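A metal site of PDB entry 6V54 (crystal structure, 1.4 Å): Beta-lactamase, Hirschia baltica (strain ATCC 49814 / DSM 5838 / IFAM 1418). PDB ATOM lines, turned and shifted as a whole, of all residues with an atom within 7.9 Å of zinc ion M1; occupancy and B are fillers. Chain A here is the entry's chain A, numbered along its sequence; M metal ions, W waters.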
ATOM      1  N   THR A  89      17.459  -6.972 -22.661  1.00  0.00           N
ATOM      2  CA  THR A  89      18.549  -6.136 -22.184  1.00  0.00           C
ATOM      3  C   THR A  89      19.589  -5.764 -23.220  1.00  0.00           C
ATOM      4  O   THR A  89      20.379  -4.877 -22.943  1.00  0.00           O
ATOM      5  CB  THR A  89      19.155  -6.687 -20.879  1.00  0.00           C
ATOM      6  OG1 THR A  89      19.675  -8.010 -21.101  1.00  0.00           O
ATOM      7  CG2 THR A  89      18.052  -6.757 -19.810  1.00  0.00           C
ATOM      8  N   HIS A  90      19.626  -6.426 -24.386  1.00  0.00           N
ATOM      9  CA  HIS A  90      20.336  -5.916 -25.567  1.00  0.00           C
ATOM     10  C   HIS A  90      20.029  -6.855 -26.726  1.00  0.00           C
ATOM     11  O   HIS A  90      19.445  -7.933 -26.544  1.00  0.00           O
ATOM     12  CB  HIS A  90      21.855  -5.763 -25.374  1.00  0.00           C
ATOM     13  CG  HIS A  90      22.592  -7.049 -25.221  1.00  0.00           C
ATOM     14  ND1 HIS A  90      22.631  -7.743 -24.028  1.00  0.00           N
ATOM     15  CD2 HIS A  90      23.369  -7.736 -26.085  1.00  0.00           C
ATOM     16  CE1 HIS A  90      23.337  -8.849 -24.192  1.00  0.00           C
ATOM     17  NE2 HIS A  90      23.796  -8.871 -25.442  1.00  0.00           N
ATOM     18  N   ALA A  91      20.454  -6.432 -27.913  1.00  0.00           N
ATOM     19  CA  ALA A  91      20.103  -7.119 -29.166  1.00  0.00           C
ATOM     20  C   ALA A  91      21.145  -8.190 -29.523  1.00  0.00           C
ATOM     21  O   ALA A  91      21.964  -8.028 -30.429  1.00  0.00           O
ATOM     22  CB  ALA A  91      19.992  -6.095 -30.290  1.00  0.00           C
ATOM     23  N   HIS A  92      21.089  -9.322 -28.796  1.00  0.00           N
ATOM     24  CA  HIS A  92      21.810 -10.544 -29.153  1.00  0.00           C
ATOM     25  C   HIS A  92      20.862 -11.713 -28.970  1.00  0.00           C
ATOM     26  O   HIS A  92      19.865 -11.614 -28.251  1.00  0.00           O
ATOM     27  CB  HIS A  92      23.075 -10.740 -28.288  1.00  0.00           C
ATOM     28  CG  HIS A  92      24.281  -9.965 -28.747  1.00  0.00           C
ATOM     29  ND1 HIS A  92      25.370  -9.673 -27.920  1.00  0.00           N
ATOM     30  CD2 HIS A  92      24.590  -9.467 -29.966  1.00  0.00           C
ATOM     31  CE1 HIS A  92      26.291  -9.029 -28.624  1.00  0.00           C
ATOM     32  NE2 HIS A  92      25.851  -8.909 -29.863  1.00  0.00           N
ATOM     33  N   SER A  93      21.216 -12.857 -29.544  1.00  0.00           N
ATOM     34  CA  SER A  93      20.279 -13.972 -29.594  1.00  0.00           C
ATOM     35  C   SER A  93      20.092 -14.680 -28.238  1.00  0.00           C
ATOM     36  O   SER A  93      19.121 -15.420 -28.061  1.00  0.00           O
ATOM     37  CB  SER A  93      20.658 -14.967 -30.676  1.00  0.00           C
ATOM     38  OG  SER A  93      21.828 -15.657 -30.313  1.00  0.00           O
ATOM     39  N   ASP A  94      20.995 -14.507 -27.294  1.00  0.00           N
ATOM     40  CA  ASP A  94      20.735 -15.050 -25.961  1.00  0.00           C
ATOM     41  C   ASP A  94      19.667 -14.268 -25.215  1.00  0.00           C
ATOM     42  O   ASP A  94      19.109 -14.800 -24.232  1.00  0.00           O
ATOM     43  CB  ASP A  94      22.000 -15.182 -25.101  1.00  0.00           C
ATOM     44  CG  ASP A  94      22.867 -13.948 -25.081  1.00  0.00           C
ATOM     45  OD1 ASP A  94      22.849 -13.069 -25.950  1.00  0.00           O
ATOM     46  OD2 ASP A  94      23.672 -13.891 -24.171  1.00  0.00           O
ATOM     47  N   LYS A  95      19.390 -13.025 -25.607  1.00  0.00           N
ATOM     48  CA  LYS A  95      18.429 -12.181 -24.920  1.00  0.00           C
ATOM     49  C   LYS A  95      17.148 -12.022 -25.703  1.00  0.00           C
ATOM     50  O   LYS A  95      16.107 -11.646 -25.120  1.00  0.00           O
ATOM     51  CB  LYS A  95      19.029 -10.776 -24.696  1.00  0.00           C
ATOM     52  CG  LYS A  95      20.483 -10.695 -24.172  1.00  0.00           C
ATOM     53  CD  LYS A  95      20.553 -10.944 -22.661  1.00  0.00           C
ATOM     54  CE  LYS A  95      20.532 -12.414 -22.224  1.00  0.00           C
ATOM     55  NZ  LYS A  95      20.410 -12.449 -20.696  1.00  0.00           N
ATOM     56  N   ARG A 122      20.717  -6.890 -36.795  1.00  0.00           N
ATOM     57  CA  ARG A 122      21.352  -8.160 -36.472  1.00  0.00           C
ATOM     58  C   ARG A 122      20.482  -9.360 -36.822  1.00  0.00           C
ATOM     59  O   ARG A 122      20.850 -10.499 -36.497  1.00  0.00           O
ATOM     60  CB  ARG A 122      21.768  -8.166 -34.983  1.00  0.00           C
ATOM     61  CG  ARG A 122      22.819  -7.104 -34.686  1.00  0.00           C
ATOM     62  CD  ARG A 122      23.014  -6.853 -33.199  1.00  0.00           C
ATOM     63  NE  ARG A 122      23.970  -5.750 -32.995  1.00  0.00           N
ATOM     64  CZ  ARG A 122      24.367  -5.324 -31.785  1.00  0.00           C
ATOM     65  NH1 ARG A 122      23.929  -5.924 -30.662  1.00  0.00           N
ATOM     66  NH2 ARG A 122      25.236  -4.323 -31.706  1.00  0.00           N
ATOM     67  N   HIS A 154      29.139  -4.150 -23.163  1.00  0.00           N
ATOM     68  CA  HIS A 154      29.187  -5.380 -23.941  1.00  0.00           C
ATOM     69  C   HIS A 154      28.528  -5.173 -25.307  1.00  0.00           C
ATOM     70  O   HIS A 154      28.971  -5.745 -26.324  1.00  0.00           O
ATOM     71  CB  HIS A 154      28.395  -6.447 -23.148  1.00  0.00           C
ATOM     72  CG  HIS A 154      27.969  -7.607 -23.967  1.00  0.00           C
ATOM     73  ND1 HIS A 154      28.837  -8.609 -24.330  1.00  0.00           N
ATOM     74  CD2 HIS A 154      26.775  -7.892 -24.554  1.00  0.00           C
ATOM     75  CE1 HIS A 154      28.182  -9.479 -25.094  1.00  0.00           C
ATOM     76  NE2 HIS A 154      26.938  -9.072 -25.233  1.00  0.00           N
ATOM     77  N   SER A 155      27.452  -4.381 -25.343  1.00  0.00           N
ATOM     78  CA  SER A 155      26.827  -3.959 -26.591  1.00  0.00           C
ATOM     79  C   SER A 155      26.431  -2.513 -26.388  1.00  0.00           C
ATOM     80  O   SER A 155      26.289  -2.071 -25.245  1.00  0.00           O
ATOM     81  CB  SER A 155      25.590  -4.848 -26.871  1.00  0.00           C
ATOM     82  OG  SER A 155      25.019  -4.560 -28.149  1.00  0.00           O
ATOM     83  N   ASP A 157      23.844  -0.888 -26.740  1.00  0.00           N
ATOM     84  CA  ASP A 157      22.487  -0.670 -26.243  1.00  0.00           C
ATOM     85  C   ASP A 157      22.243  -1.319 -24.881  1.00  0.00           C
ATOM     86  O   ASP A 157      21.105  -1.265 -24.395  1.00  0.00           O
ATOM     87  CB  ASP A 157      21.502  -1.289 -27.256  1.00  0.00           C
ATOM     88  CG  ASP A 157      21.774  -2.793 -27.523  1.00  0.00           C
ATOM     89  OD1 ASP A 157      22.964  -3.227 -27.588  1.00  0.00           O
ATOM     90  OD2 ASP A 157      20.790  -3.540 -27.643  1.00  0.00           O
ATOM     91  N   ASN A 158      23.246  -1.948 -24.265  1.00  0.00           N
ATOM     92  CA  ASN A 158      22.957  -2.751 -23.073  1.00  0.00           C
ATOM     93  C   ASN A 158      22.280  -1.907 -21.972  1.00  0.00           C
ATOM     94  O   ASN A 158      22.704  -0.782 -21.678  1.00  0.00           O
ATOM     95  CB  ASN A 158      24.221  -3.541 -22.575  1.00  0.00           C
ATOM     96  CG  ASN A 158      25.497  -2.728 -22.347  1.00  0.00           C
ATOM     97  OD1 ASN A 158      26.574  -3.356 -22.335  1.00  0.00           O
ATOM     98  ND2 ASN A 158      25.411  -1.410 -22.075  1.00  0.00           N
ATOM     99  N   GLY A 172      22.998  -8.648 -16.763  1.00  0.00           N
ATOM    100  CA  GLY A 172      23.023  -9.241 -18.087  1.00  0.00           C
ATOM    101  C   GLY A 172      24.444  -9.456 -18.573  1.00  0.00           C
ATOM    102  O   GLY A 172      25.357  -9.791 -17.792  1.00  0.00           O
ATOM    103  N   CYS A 173      24.656  -9.247 -19.874  1.00  0.00           N
ATOM    104  CA  CYS A 173      25.939  -9.604 -20.437  1.00  0.00           C
ATOM    105  C   CYS A 173      26.994  -8.521 -20.232  1.00  0.00           C
ATOM    106  O   CYS A 173      28.187  -8.775 -20.499  1.00  0.00           O
ATOM    107  CB  CYS A 173      25.797  -9.885 -21.924  1.00  0.00           C
ATOM    108  SG  CYS A 173      24.583 -11.212 -22.255  1.00  0.00           S
ATOM    109  N   MET A 174      26.582  -7.379 -19.710  1.00  0.00           N
ATOM    110  CA  MET A 174      27.531  -6.319 -19.423  1.00  0.00           C
ATOM    111  C   MET A 174      28.407  -6.707 -18.233  1.00  0.00           C
ATOM    112  O   MET A 174      29.488  -6.156 -18.067  1.00  0.00           O
ATOM    113  CB  MET A 174      26.766  -5.055 -19.065  1.00  0.00           C
ATOM    114  CG  MET A 174      27.644  -3.789 -19.121  1.00  0.00           C
ATOM    115  SD  MET A 174      26.604  -2.221 -18.750  1.00  0.00           S
ATOM    116  CE  MET A 174      26.717  -2.274 -16.919  1.00  0.00           C
ATOM    117  N   ASN A 185      31.987 -12.464 -25.838  1.00  0.00           N
ATOM    118  CA  ASN A 185      31.740 -12.023 -27.208  1.00  0.00           C
ATOM    119  C   ASN A 185      31.855 -10.511 -27.277  1.00  0.00           C
ATOM    120  O   ASN A 185      30.969  -9.806 -26.804  1.00  0.00           O
ATOM    121  CB  ASN A 185      30.337 -12.479 -27.633  1.00  0.00           C
ATOM    122  CG  ASN A 185      29.908 -11.888 -28.973  1.00  0.00           C
ATOM    123  OD1 ASN A 185      30.725 -11.321 -29.710  1.00  0.00           O
ATOM    124  ND2 ASN A 185      28.612 -12.005 -29.278  1.00  0.00           N
ATOM    125  N   ILE A 186      32.921 -10.014 -27.911  1.00  0.00           N
ATOM    126  CA  ILE A 186      33.170  -8.575 -27.981  1.00  0.00           C
ATOM    127  C   ILE A 186      32.870  -8.005 -29.357  1.00  0.00           C
ATOM    128  O   ILE A 186      33.262  -6.865 -29.634  1.00  0.00           O
ATOM    129  CB  ILE A 186      34.574  -8.173 -27.507  1.00  0.00           C
ATOM    130  CG1 ILE A 186      35.697  -9.001 -28.167  1.00  0.00           C
ATOM    131  CG2 ILE A 186      34.697  -8.377 -26.022  1.00  0.00           C
ATOM    132  CD1 ILE A 186      35.808  -8.949 -29.703  1.00  0.00           C
ATOM    133  N   ASP A 188      30.418  -6.682 -30.676  1.00  0.00           N
ATOM    134  CA  ASP A 188      29.629  -5.452 -30.682  1.00  0.00           C
ATOM    135  C   ASP A 188      29.957  -4.560 -29.484  1.00  0.00           C
ATOM    136  O   ASP A 188      29.219  -3.619 -29.195  1.00  0.00           O
ATOM    137  CB  ASP A 188      28.142  -5.825 -30.696  1.00  0.00           C
ATOM    138  CG  ASP A 188      27.767  -6.550 -31.990  1.00  0.00           C
ATOM    139  OD1 ASP A 188      28.223  -6.102 -33.078  1.00  0.00           O
ATOM    140  OD2 ASP A 188      27.041  -7.554 -31.930  1.00  0.00           O
ATOM    141  N   SER A 214      24.726 -12.685 -17.179  1.00  0.00           N
ATOM    142  CA  SER A 214      24.033 -13.625 -18.059  1.00  0.00           C
ATOM    143  C   SER A 214      24.716 -14.964 -18.167  1.00  0.00           C
ATOM    144  O   SER A 214      24.026 -15.973 -18.374  1.00  0.00           O
ATOM    145  CB  SER A 214      23.947 -13.119 -19.486  1.00  0.00           C
ATOM    146  OG  SER A 214      23.076 -12.014 -19.602  1.00  0.00           O
ATOM    147  N   HIS A 215      26.051 -15.008 -18.111  1.00  0.00           N
ATOM    148  CA  HIS A 215      26.791 -16.201 -18.522  1.00  0.00           C
ATOM    149  C   HIS A 215      27.546 -16.867 -17.374  1.00  0.00           C
ATOM    150  O   HIS A 215      28.546 -17.542 -17.605  1.00  0.00           O
ATOM    151  CB  HIS A 215      27.700 -15.911 -19.718  1.00  0.00           C
ATOM    152  CG  HIS A 215      26.939 -15.427 -20.929  1.00  0.00           C
ATOM    153  ND1 HIS A 215      25.948 -16.175 -21.530  1.00  0.00           N
ATOM    154  CD2 HIS A 215      27.005 -14.257 -21.610  1.00  0.00           C
ATOM    155  CE1 HIS A 215      25.444 -15.505 -22.550  1.00  0.00           C
ATOM    156  NE2 HIS A 215      26.074 -14.334 -22.635  1.00  0.00           N
HETATM  157 ZN    ZN M   1      25.359 -10.060 -25.974  1.00  0.00          ZN
HETATM  158 ZN    ZN M   2      25.349 -12.742 -23.682  1.00  0.00          ZN
HETATM  159  O   HOH W   1      25.344 -11.979 -25.612  1.00  0.00           O
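OD1 of Asn 158 is in hydrogen-bond range of N of His 154. OG of Ser 214 sits at hydrogen-bond distance from N of Cys 173 (3.2 Å). NE2 of His 92 lies within hydrogen-bond range of OD2 of Asp 188 (2.7 Å). O of Asn 185 lies close to ND1 of His 154 (3.5 Å).
Residues that only touch zinc ion M1: Asp 94 and Cys 173. Five residues have an atom within 4 Å of zinc ion M1: His 90, His 92, Asp 94, His 154 and Cys 173. The nearest printed residue that does not touch zinc ion M1 is Asn 185 (5.0 Å).
Water W1 binds zinc ion M1 (2.0 Å). A ring nitrogen (ND1) of His 92 binds zinc ion M1 (2.0 Å). NE2 of His 154 is bound to zinc ion M1 (2.0 Å). Zinc ion M1 is bound by NE2 of His 90, 2.0 Å away.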
